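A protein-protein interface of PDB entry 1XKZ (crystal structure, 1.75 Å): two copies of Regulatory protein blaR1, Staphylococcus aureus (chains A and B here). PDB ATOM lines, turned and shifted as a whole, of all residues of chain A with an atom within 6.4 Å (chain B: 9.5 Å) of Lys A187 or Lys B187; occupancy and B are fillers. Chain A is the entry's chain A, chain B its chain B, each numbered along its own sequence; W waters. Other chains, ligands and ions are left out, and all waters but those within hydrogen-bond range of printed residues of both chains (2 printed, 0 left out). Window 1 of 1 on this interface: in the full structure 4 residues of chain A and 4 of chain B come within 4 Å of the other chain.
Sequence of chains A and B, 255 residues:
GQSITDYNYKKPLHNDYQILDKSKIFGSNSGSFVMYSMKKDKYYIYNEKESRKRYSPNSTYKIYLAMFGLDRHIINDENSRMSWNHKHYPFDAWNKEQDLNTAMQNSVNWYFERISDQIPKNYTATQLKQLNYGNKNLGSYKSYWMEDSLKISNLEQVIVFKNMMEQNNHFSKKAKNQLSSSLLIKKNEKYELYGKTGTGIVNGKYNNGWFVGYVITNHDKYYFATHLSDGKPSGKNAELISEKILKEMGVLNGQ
Hydrophobic or aromatic side chains of chain B that line the printed part of chain A: Leu B184.
Of the 11 printed residues of chain A, 4 touch a printed residue of chain B.
Water W1 lies within hydrogen-bond range of OE1 of Gln B105 (2.6 Å) and NZ of Lys A187 (2.9 Å).
Water W2 lies within hydrogen-bond range of the side-chain amide oxygen (OE1) of Gln A105 and the side-chain amino group (NZ) of Lys B187.
N of Lys B187 is in hydrogen-bond range of O of Lys A187 (2.9 Å).
Of the printed residues of chain B, Leu A184 touches Leu B184 (3.6 Å) and Lys B187 (3.4 Å).
Lys A187 touches just these residues of chain B: Leu B184 (3.3 Å), Ile B185 (3.6 Å), Lys B186 (3.3 Å) and Lys B187 (2.9 Å).
No residue of chain B comes within 4 Å of Asn A188.
Of the printed residues of chain A, Leu B184 touches Leu A184 (3.6 Å) and Lys A187 (3.3 Å).
Of the printed residues of chain A, Ile B185 touches Lys A187 (3.6 Å).
Printed residues of chain A within 4 Å of Lys B186: Lys A187 (3.3 Å).
Lys B187 touches four residues of chain A.
The nearest residue of chain B that does not touch Lys A187 is Gln B105 (4.5 Å).
Leu A184 touches Leu B184 (CD2 to CD2, 3.6 Å).
Leu A184 touches Lys B187 (O to CE, 3.4 Å).
Lys B187 touches Ile A185.
Lys B187 touches Lys A186.
CE of Lys A187 touches O of Leu B184, 3.3 Å away.
O of Ile B185 touches CG of Lys A187, at 3.6 Å.
Lys B186 touches Lys A187 (CA to O, 3.3 Å).
The backbone NH (N) of Ile B185 is in hydrogen-bond range of the backbone carbonyl oxygen (O) of Leu B193.
The side-chain amino group (NZ) of Lys B187 lies within salt-bridge range of the side-chain carboxylate (OE2) of Glu B192, at 2.7 Å.
O of Lys A186 is in hydrogen-bond range of N of Leu A193 (2.7 Å).
The side-chain amino group of Lys A187 is in salt-bridge range of the side-chain carboxylate of Glu A192.
NZ of Lys A186 lies close to OH of Tyr A191 (3.3 Å).
The backbone carbonyl oxygen (O) of Leu A193 sits at hydrogen-bond distance from the backbone NH (N) of Ile A185 (2.8 Å).
Leu A184 touches Lys B187, and with the chains exchanged Lys A187 touches Leu B184.
Ile A185 touches Lys B187, and with the chains exchanged Lys A187 touches Ile B185.
Lys A186 touches Lys B187, and with the chains exchanged Lys A187 touches Lys B186.
Lys A187 touches its own counterpart, Lys B187.
Positions printed for both chains: 105, 184, 185, 186, 187, 188, 189, 190, 191, 192 and 193.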
ATOM      1  N   GLN A 105      36.162 -11.130 -21.623  1.00  0.00           N
ATOM      2  CA  GLN A 105      36.662 -10.579 -20.351  1.00  0.00           C
ATOM      3  C   GLN A 105      38.183 -10.464 -20.280  1.00  0.00           C
ATOM      4  O   GLN A 105      38.748  -9.455 -19.766  1.00  0.00           O
ATOM      5  CB  GLN A 105      36.152 -11.406 -19.151  1.00  0.00           C
ATOM      6  CG  GLN A 105      36.785 -11.056 -17.810  1.00  0.00           C
ATOM      7  CD  GLN A 105      36.380 -11.965 -16.639  1.00  0.00           C
ATOM      8  OE1 GLN A 105      35.289 -12.539 -16.604  1.00  0.00           O
ATOM      9  NE2 GLN A 105      37.255 -12.051 -15.655  1.00  0.00           N
ATOM     10  N   LEU A 184      29.237  -7.431 -19.926  1.00  0.00           N
ATOM     11  CA  LEU A 184      28.937  -6.938 -18.570  1.00  0.00           C
ATOM     12  C   LEU A 184      30.154  -6.910 -17.620  1.00  0.00           C
ATOM     13  O   LEU A 184      30.849  -7.929 -17.426  1.00  0.00           O
ATOM     14  CB  LEU A 184      27.722  -7.721 -17.953  1.00  0.00           C
ATOM     15  CG  LEU A 184      27.335  -7.266 -16.543  1.00  0.00           C
ATOM     16  CD1 LEU A 184      26.644  -5.916 -16.549  1.00  0.00           C
ATOM     17  CD2 LEU A 184      26.392  -8.269 -15.920  1.00  0.00           C
ATOM     18  N   ILE A 185      30.426  -5.729 -17.053  1.00  0.00           N
ATOM     19  CA  ILE A 185      31.563  -5.529 -16.172  1.00  0.00           C
ATOM     20  C   ILE A 185      31.164  -5.287 -14.731  1.00  0.00           C
ATOM     21  O   ILE A 185      31.776  -5.827 -13.768  1.00  0.00           O
ATOM     22  CB  ILE A 185      32.455  -4.307 -16.655  1.00  0.00           C
ATOM     23  CG1 ILE A 185      32.941  -4.476 -18.105  1.00  0.00           C
ATOM     24  CG2 ILE A 185      33.579  -3.995 -15.683  1.00  0.00           C
ATOM     25  CD1 ILE A 185      33.833  -5.622 -18.398  1.00  0.00           C
ATOM     26  N   LYS A 186      30.182  -4.411 -14.568  1.00  0.00           N
ATOM     27  CA  LYS A 186      29.727  -4.047 -13.257  1.00  0.00           C
ATOM     28  C   LYS A 186      28.218  -3.977 -13.151  1.00  0.00           C
ATOM     29  O   LYS A 186      27.528  -3.616 -14.106  1.00  0.00           O
ATOM     30  CB  LYS A 186      30.360  -2.695 -12.871  1.00  0.00           C
ATOM     31  CG  LYS A 186      30.381  -2.446 -11.406  1.00  0.00           C
ATOM     32  CD  LYS A 186      31.679  -1.721 -11.020  1.00  0.00           C
ATOM     33  CE  LYS A 186      31.422  -0.546 -10.125  1.00  0.00           C
ATOM     34  NZ  LYS A 186      30.473  -0.879  -8.997  1.00  0.00           N
ATOM     35  N   LYS A 187      27.681  -4.445 -12.024  1.00  0.00           N
ATOM     36  CA  LYS A 187      26.255  -4.345 -11.804  1.00  0.00           C
ATOM     37  C   LYS A 187      26.048  -4.092 -10.342  1.00  0.00           C
ATOM     38  O   LYS A 187      26.744  -4.690  -9.493  1.00  0.00           O
ATOM     39  CB  LYS A 187      25.479  -5.644 -12.214  1.00  0.00           C
ATOM     40  CG  LYS A 187      23.973  -5.619 -11.913  1.00  0.00           C
ATOM     41  CD  LYS A 187      23.276  -6.807 -12.597  1.00  0.00           C
ATOM     42  CE  LYS A 187      21.748  -6.917 -12.311  1.00  0.00           C
ATOM     43  NZ  LYS A 187      20.845  -5.779 -12.777  1.00  0.00           N
ATOM     44  N   ASN A 188      25.208  -3.096 -10.068  1.00  0.00           N
ATOM     45  CA  ASN A 188      24.809  -2.780  -8.713  1.00  0.00           C
ATOM     46  C   ASN A 188      23.358  -2.346  -8.695  1.00  0.00           C
ATOM     47  O   ASN A 188      22.654  -2.513  -9.696  1.00  0.00           O
ATOM     48  CB  ASN A 188      25.817  -1.856  -7.963  1.00  0.00           C
ATOM     49  CG  ASN A 188      25.771  -0.414  -8.397  1.00  0.00           C
ATOM     50  OD1 ASN A 188      26.633   0.414  -8.004  1.00  0.00           O
ATOM     51  ND2 ASN A 188      24.795  -0.083  -9.190  1.00  0.00           N
ATOM     52  N   GLU A 189      22.898  -1.798  -7.570  1.00  0.00           N
ATOM     53  CA  GLU A 189      21.494  -1.357  -7.406  1.00  0.00           C
ATOM     54  C   GLU A 189      21.069  -0.286  -8.394  1.00  0.00           C
ATOM     55  O   GLU A 189      19.916  -0.206  -8.792  1.00  0.00           O
ATOM     56  CB  GLU A 189      21.294  -0.776  -5.984  1.00  0.00           C
ATOM     57  N   LYS A 190      22.049   0.516  -8.767  1.00  0.00           N
ATOM     58  CA  LYS A 190      21.872   1.703  -9.628  1.00  0.00           C
ATOM     59  C   LYS A 190      22.113   1.527 -11.116  1.00  0.00           C
ATOM     60  O   LYS A 190      21.499   2.223 -11.931  1.00  0.00           O
ATOM     61  CB  LYS A 190      22.817   2.771  -9.116  1.00  0.00           C
ATOM     62  N   TYR A 191      23.015   0.615 -11.476  1.00  0.00           N
ATOM     63  CA  TYR A 191      23.322   0.471 -12.888  1.00  0.00           C
ATOM     64  C   TYR A 191      23.990  -0.823 -13.278  1.00  0.00           C
ATOM     65  O   TYR A 191      24.580  -1.513 -12.420  1.00  0.00           O
ATOM     66  CB  TYR A 191      24.253   1.647 -13.328  1.00  0.00           C
ATOM     67  CG  TYR A 191      25.651   1.672 -12.653  1.00  0.00           C
ATOM     68  CD1 TYR A 191      26.732   0.936 -13.198  1.00  0.00           C
ATOM     69  CD2 TYR A 191      25.877   2.387 -11.458  1.00  0.00           C
ATOM     70  CE1 TYR A 191      27.997   0.912 -12.570  1.00  0.00           C
ATOM     71  CE2 TYR A 191      27.166   2.371 -10.815  1.00  0.00           C
ATOM     72  CZ  TYR A 191      28.197   1.636 -11.383  1.00  0.00           C
ATOM     73  OH  TYR A 191      29.441   1.630 -10.821  1.00  0.00           O
ATOM     74  N   GLU A 192      24.029  -1.048 -14.592  1.00  0.00           N
ATOM     75  CA  GLU A 192      24.779  -2.176 -15.190  1.00  0.00           C
ATOM     76  C   GLU A 192      25.744  -1.481 -16.182  1.00  0.00           C
ATOM     77  O   GLU A 192      25.279  -0.724 -17.072  1.00  0.00           O
ATOM     78  CB  GLU A 192      23.884  -3.093 -16.000  1.00  0.00           C
ATOM     79  CG  GLU A 192      22.947  -3.918 -15.186  1.00  0.00           C
ATOM     80  CD  GLU A 192      22.072  -4.841 -16.047  1.00  0.00           C
ATOM     81  OE1 GLU A 192      21.935  -4.630 -17.271  1.00  0.00           O
ATOM     82  OE2 GLU A 192      21.481  -5.778 -15.479  1.00  0.00           O
ATOM     83  N   LEU A 193      27.039  -1.780 -16.073  1.00  0.00           N
ATOM     84  CA  LEU A 193      28.052  -1.193 -16.964  1.00  0.00           C
ATOM     85  C   LEU A 193      28.594  -2.299 -17.874  1.00  0.00           C
ATOM     86  O   LEU A 193      29.040  -3.341 -17.406  1.00  0.00           O
ATOM     87  CB  LEU A 193      29.181  -0.583 -16.133  1.00  0.00           C
ATOM     88  CG  LEU A 193      30.487  -0.187 -16.852  1.00  0.00           C
ATOM     89  CD1 LEU A 193      30.208   1.034 -17.675  1.00  0.00           C
ATOM     90  CD2 LEU A 193      31.556   0.118 -15.867  1.00  0.00           C
ATOM     91  N   ASN B 101      13.757 -11.565 -16.438  1.00  0.00           N
ATOM     92  CA  ASN B 101      14.587 -10.688 -15.629  1.00  0.00           C
ATOM     93  C   ASN B 101      13.828  -9.613 -14.839  1.00  0.00           C
ATOM     94  O   ASN B 101      14.109  -9.418 -13.654  1.00  0.00           O
ATOM     95  CB  ASN B 101      15.676 -10.025 -16.480  1.00  0.00           C
ATOM     96  CG  ASN B 101      16.700 -11.012 -17.033  1.00  0.00           C
ATOM     97  OD1 ASN B 101      16.853 -12.122 -16.536  1.00  0.00           O
ATOM     98  ND2 ASN B 101      17.312 -10.642 -18.172  1.00  0.00           N
ATOM     99  N   THR B 102      12.825  -8.984 -15.469  1.00  0.00           N
ATOM    100  CA  THR B 102      12.063  -7.973 -14.760  1.00  0.00           C
ATOM    101  C   THR B 102      11.212  -8.591 -13.698  1.00  0.00           C
ATOM    102  O   THR B 102      11.098  -8.049 -12.606  1.00  0.00           O
ATOM    103  CB  THR B 102      11.223  -7.053 -15.698  1.00  0.00           C
ATOM    104  OG1 THR B 102      10.141  -7.795 -16.271  1.00  0.00           O
ATOM    105  CG2 THR B 102      12.145  -6.464 -16.807  1.00  0.00           C
ATOM    106  N   GLN B 105      13.541  -9.704 -10.669  1.00  0.00           N
ATOM    107  CA  GLN B 105      14.076  -8.546  -9.990  1.00  0.00           C
ATOM    108  C   GLN B 105      13.054  -7.796  -9.165  1.00  0.00           C
ATOM    109  O   GLN B 105      13.325  -7.414  -8.035  1.00  0.00           O
ATOM    110  CB  GLN B 105      14.698  -7.585 -11.026  1.00  0.00           C
ATOM    111  CG  GLN B 105      15.276  -6.280 -10.405  1.00  0.00           C
ATOM    112  CD  GLN B 105      15.590  -5.256 -11.461  1.00  0.00           C
ATOM    113  OE1 GLN B 105      16.368  -5.508 -12.358  1.00  0.00           O
ATOM    114  NE2 GLN B 105      14.868  -4.125 -11.429  1.00  0.00           N
ATOM    115  N   SER B 180      20.320 -18.120 -13.918  1.00  0.00           N
ATOM    116  CA  SER B 180      21.370 -17.372 -13.229  1.00  0.00           C
ATOM    117  C   SER B 180      21.375 -15.900 -13.567  1.00  0.00           C
ATOM    118  O   SER B 180      21.479 -15.079 -12.673  1.00  0.00           O
ATOM    119  CB  SER B 180      22.730 -17.918 -13.562  1.00  0.00           C
ATOM    120  OG  SER B 180      22.812 -19.134 -12.872  1.00  0.00           O
ATOM    121  N   SER B 181      21.227 -15.607 -14.862  1.00  0.00           N
ATOM    122  CA  SER B 181      21.196 -14.208 -15.328  1.00  0.00           C
ATOM    123  C   SER B 181      20.086 -13.425 -14.656  1.00  0.00           C
ATOM    124  O   SER B 181      20.290 -12.279 -14.250  1.00  0.00           O
ATOM    125  CB  SER B 181      20.974 -14.154 -16.835  1.00  0.00           C
ATOM    126  OG  SER B 181      22.099 -14.680 -17.517  1.00  0.00           O
ATOM    127  N   SER B 182      18.930 -14.079 -14.440  1.00  0.00           N
ATOM    128  CA  SER B 182      17.816 -13.410 -13.790  1.00  0.00           C
ATOM    129  C   SER B 182      18.046 -13.161 -12.323  1.00  0.00           C
ATOM    130  O   SER B 182      17.415 -12.279 -11.711  1.00  0.00           O
ATOM    131  CB  SER B 182      16.492 -14.180 -14.030  1.00  0.00           C
ATOM    132  OG  SER B 182      16.381 -15.261 -13.109  1.00  0.00           O
ATOM    133  N   LEU B 183      18.949 -13.951 -11.733  1.00  0.00           N
ATOM    134  CA  LEU B 183      19.230 -13.840 -10.309  1.00  0.00           C
ATOM    135  C   LEU B 183      20.439 -12.955  -9.946  1.00  0.00           C
ATOM    136  O   LEU B 183      20.665 -12.691  -8.803  1.00  0.00           O
ATOM    137  CB  LEU B 183      19.427 -15.251  -9.711  1.00  0.00           C
ATOM    138  CG  LEU B 183      18.176 -16.136  -9.771  1.00  0.00           C
ATOM    139  CD1 LEU B 183      18.577 -17.609  -9.363  1.00  0.00           C
ATOM    140  CD2 LEU B 183      17.126 -15.538  -8.800  1.00  0.00           C
ATOM    141  N   LEU B 184      21.162 -12.452 -10.946  1.00  0.00           N
ATOM    142  CA  LEU B 184      22.338 -11.624 -10.650  1.00  0.00           C
ATOM    143  C   LEU B 184      21.939 -10.326  -9.980  1.00  0.00           C
ATOM    144  O   LEU B 184      21.031  -9.609 -10.463  1.00  0.00           O
ATOM    145  CB  LEU B 184      23.137 -11.369 -11.944  1.00  0.00           C
ATOM    146  CG  LEU B 184      24.413 -10.534 -11.760  1.00  0.00           C
ATOM    147  CD1 LEU B 184      25.472 -11.321 -10.998  1.00  0.00           C
ATOM    148  CD2 LEU B 184      24.965 -10.069 -13.166  1.00  0.00           C
ATOM    149  N   ILE B 185      22.592 -10.035  -8.858  1.00  0.00           N
ATOM    150  CA  ILE B 185      22.275  -8.810  -8.110  1.00  0.00           C
ATOM    151  C   ILE B 185      23.441  -7.824  -8.232  1.00  0.00           C
ATOM    152  O   ILE B 185      23.231  -6.638  -8.506  1.00  0.00           O
ATOM    153  CB  ILE B 185      21.972  -9.121  -6.621  1.00  0.00           C
ATOM    154  CG1 ILE B 185      20.715 -10.021  -6.466  1.00  0.00           C
ATOM    155  CG2 ILE B 185      21.865  -7.853  -5.756  1.00  0.00           C
ATOM    156  CD1 ILE B 185      19.513  -9.601  -7.182  1.00  0.00           C
ATOM    157  N   LYS B 186      24.644  -8.318  -7.958  1.00  0.00           N
ATOM    158  CA  LYS B 186      25.837  -7.460  -8.027  1.00  0.00           C
ATOM    159  C   LYS B 186      27.001  -8.151  -8.733  1.00  0.00           C
ATOM    160  O   LYS B 186      27.204  -9.357  -8.605  1.00  0.00           O
ATOM    161  CB  LYS B 186      26.235  -7.022  -6.557  1.00  0.00           C
ATOM    162  N   LYS B 187      27.776  -7.379  -9.508  1.00  0.00           N
ATOM    163  CA  LYS B 187      28.945  -7.912 -10.172  1.00  0.00           C
ATOM    164  C   LYS B 187      30.022  -6.822 -10.058  1.00  0.00           C
ATOM    165  O   LYS B 187      29.746  -5.676 -10.326  1.00  0.00           O
ATOM    166  CB  LYS B 187      28.657  -8.242 -11.619  1.00  0.00           C
ATOM    167  CG  LYS B 187      29.929  -8.647 -12.393  1.00  0.00           C
ATOM    168  CD  LYS B 187      29.663  -9.088 -13.788  1.00  0.00           C
ATOM    169  CE  LYS B 187      31.005  -9.513 -14.419  1.00  0.00           C
ATOM    170  NZ  LYS B 187      31.704 -10.713 -13.906  1.00  0.00           N
ATOM    171  N   ASN B 188      31.210  -7.171  -9.587  1.00  0.00           N
ATOM    172  CA  ASN B 188      32.306  -6.186  -9.528  1.00  0.00           C
ATOM    173  C   ASN B 188      33.582  -6.974  -9.815  1.00  0.00           C
ATOM    174  O   ASN B 188      33.512  -8.134 -10.235  1.00  0.00           O
ATOM    175  CB  ASN B 188      32.349  -5.447  -8.192  1.00  0.00           C
ATOM    176  CG  ASN B 188      32.230  -6.381  -7.031  1.00  0.00           C
ATOM    177  OD1 ASN B 188      31.134  -6.589  -6.481  1.00  0.00           O
ATOM    178  ND2 ASN B 188      33.282  -7.080  -6.772  1.00  0.00           N
ATOM    179  N   GLU B 189      34.751  -6.349  -9.627  1.00  0.00           N
ATOM    180  CA  GLU B 189      36.024  -7.010  -9.924  1.00  0.00           C
ATOM    181  C   GLU B 189      36.334  -8.209  -9.016  1.00  0.00           C
ATOM    182  O   GLU B 189      37.011  -9.141  -9.433  1.00  0.00           O
ATOM    183  CB  GLU B 189      37.200  -5.972  -9.882  1.00  0.00           C
ATOM    184  N   LYS B 190      35.711  -8.235  -7.850  1.00  0.00           N
ATOM    185  CA  LYS B 190      35.958  -9.295  -6.873  1.00  0.00           C
ATOM    186  C   LYS B 190      34.951 -10.437  -6.845  1.00  0.00           C
ATOM    187  O   LYS B 190      35.300 -11.553  -6.443  1.00  0.00           O
ATOM    188  CB  LYS B 190      36.053  -8.675  -5.496  1.00  0.00           C
ATOM    189  N   TYR B 191      33.697 -10.151  -7.191  1.00  0.00           N
ATOM    190  CA  TYR B 191      32.677 -11.201  -7.129  1.00  0.00           C
ATOM    191  C   TYR B 191      31.407 -10.915  -7.951  1.00  0.00           C
ATOM    192  O   TYR B 191      31.148  -9.770  -8.346  1.00  0.00           O
ATOM    193  CB  TYR B 191      32.294 -11.404  -5.638  1.00  0.00           C
ATOM    194  CG  TYR B 191      31.567 -10.270  -4.931  1.00  0.00           C
ATOM    195  CD1 TYR B 191      30.150 -10.109  -5.035  1.00  0.00           C
ATOM    196  CD2 TYR B 191      32.274  -9.310  -4.194  1.00  0.00           C
ATOM    197  CE1 TYR B 191      29.501  -9.001  -4.436  1.00  0.00           C
ATOM    198  CE2 TYR B 191      31.630  -8.204  -3.576  1.00  0.00           C
ATOM    199  CZ  TYR B 191      30.251  -8.050  -3.705  1.00  0.00           C
ATOM    200  OH  TYR B 191      29.602  -6.968  -3.134  1.00  0.00           O
ATOM    201  N   GLU B 192      30.584 -11.956  -8.073  1.00  0.00           N
ATOM    202  CA  GLU B 192      29.249 -11.863  -8.681  1.00  0.00           C
ATOM    203  C   GLU B 192      28.343 -12.445  -7.594  1.00  0.00           C
ATOM    204  O   GLU B 192      28.587 -13.573  -7.144  1.00  0.00           O
ATOM    205  CB  GLU B 192      29.079 -12.715  -9.931  1.00  0.00           C
ATOM    206  CG  GLU B 192      29.872 -12.299 -11.164  1.00  0.00           C
ATOM    207  CD  GLU B 192      29.696 -13.220 -12.369  1.00  0.00           C
ATOM    208  OE1 GLU B 192      29.281 -14.402 -12.209  1.00  0.00           O
ATOM    209  OE2 GLU B 192      29.973 -12.764 -13.514  1.00  0.00           O
ATOM    210  N   LEU B 193      27.335 -11.686  -7.159  1.00  0.00           N
ATOM    211  CA  LEU B 193      26.395 -12.141  -6.119  1.00  0.00           C
ATOM    212  C   LEU B 193      25.028 -12.346  -6.776  1.00  0.00           C
ATOM    213  O   LEU B 193      24.542 -11.462  -7.478  1.00  0.00           O
ATOM    214  CB  LEU B 193      26.242 -11.112  -4.994  1.00  0.00           C
ATOM    215  CG  LEU B 193      25.115 -11.417  -4.003  1.00  0.00           C
ATOM    216  CD1 LEU B 193      25.690 -12.315  -2.994  1.00  0.00           C
ATOM    217  CD2 LEU B 193      24.598 -10.143  -3.370  1.00  0.00           C
ATOM    218  N   TYR B 194      24.447 -13.535  -6.550  1.00  0.00           N
ATOM    219  CA  TYR B 194      23.133 -13.879  -7.123  1.00  0.00           C
ATOM    220  C   TYR B 194      22.228 -14.191  -5.966  1.00  0.00           C
ATOM    221  O   TYR B 194      22.682 -14.632  -4.902  1.00  0.00           O
ATOM    222  CB  TYR B 194      23.216 -15.156  -7.991  1.00  0.00           C
ATOM    223  CG  TYR B 194      24.177 -15.109  -9.176  1.00  0.00           C
ATOM    224  CD1 TYR B 194      25.569 -15.204  -8.989  1.00  0.00           C
ATOM    225  CD2 TYR B 194      23.682 -14.973 -10.478  1.00  0.00           C
ATOM    226  CE1 TYR B 194      26.438 -15.142 -10.089  1.00  0.00           C
ATOM    227  CE2 TYR B 194      24.535 -14.898 -11.577  1.00  0.00           C
ATOM    228  CZ  TYR B 194      25.914 -14.981 -11.368  1.00  0.00           C
ATOM    229  OH  TYR B 194      26.702 -14.894 -12.488  1.00  0.00           O
ATOM    230  N   GLY B 195      20.930 -13.978  -6.155  1.00  0.00           N
ATOM    231  CA  GLY B 195      20.065 -14.317  -5.053  1.00  0.00           C
ATOM    232  C   GLY B 195      18.629 -13.917  -5.237  1.00  0.00           C
ATOM    233  O   GLY B 195      18.303 -13.264  -6.243  1.00  0.00           O
ATOM    234  N   VAL B 215      27.417 -16.925  -4.449  1.00  0.00           N
ATOM    235  CA  VAL B 215      28.449 -15.909  -4.751  1.00  0.00           C
ATOM    236  C   VAL B 215      29.536 -16.624  -5.498  1.00  0.00           C
ATOM    237  O   VAL B 215      30.026 -17.660  -5.017  1.00  0.00           O
ATOM    238  CB  VAL B 215      29.157 -15.391  -3.452  1.00  0.00           C
ATOM    239  CG1 VAL B 215      30.073 -14.163  -3.790  1.00  0.00           C
ATOM    240  CG2 VAL B 215      28.214 -15.012  -2.422  1.00  0.00           C
ATOM    241  N   ILE B 216      30.044 -15.992  -6.561  1.00  0.00           N
ATOM    242  CA  ILE B 216      31.165 -16.550  -7.329  1.00  0.00           C
ATOM    243  C   ILE B 216      32.319 -15.550  -7.116  1.00  0.00           C
ATOM    244  O   ILE B 216      32.176 -14.387  -7.458  1.00  0.00           O
ATOM    245  CB  ILE B 216      30.896 -16.615  -8.846  1.00  0.00           C
ATOM    246  CG1 ILE B 216      29.733 -17.552  -9.163  1.00  0.00           C
ATOM    247  CG2 ILE B 216      32.185 -17.068  -9.605  1.00  0.00           C
ATOM    248  CD1 ILE B 216      29.407 -17.645 -10.663  1.00  0.00           C
ATOM    249  N   THR B 217      33.424 -15.997  -6.527  1.00  0.00           N
ATOM    250  CA  THR B 217      34.598 -15.127  -6.304  1.00  0.00           C
ATOM    251  C   THR B 217      35.696 -15.689  -7.198  1.00  0.00           C
ATOM    252  O   THR B 217      35.492 -16.674  -7.886  1.00  0.00           O
ATOM    253  CB  THR B 217      35.073 -15.124  -4.826  1.00  0.00           C
ATOM    254  OG1 THR B 217      35.739 -16.356  -4.517  1.00  0.00           O
ATOM    255  CG2 THR B 217      33.917 -14.961  -3.883  1.00  0.00           C
ATOM    256  N   ASN B 218      36.876 -15.062  -7.207  1.00  0.00           N
ATOM    257  CA  ASN B 218      37.963 -15.562  -8.037  1.00  0.00           C
ATOM    258  C   ASN B 218      38.564 -16.861  -7.485  1.00  0.00           C
ATOM    259  O   ASN B 218      39.177 -17.631  -8.218  1.00  0.00           O
ATOM    260  CB  ASN B 218      39.051 -14.488  -8.167  1.00  0.00           C
ATOM    261  CG  ASN B 218      38.580 -13.270  -8.969  1.00  0.00           C
ATOM    262  OD1 ASN B 218      37.964 -13.421 -10.041  1.00  0.00           O
ATOM    263  ND2 ASN B 218      38.890 -12.062  -8.473  1.00  0.00           N
HETATM  264  O   HOH W   1      18.361  -7.129 -12.203  1.00  0.00           O
HETATM  265  O   HOH W   2      33.024 -11.072 -16.636  1.00  0.00           O
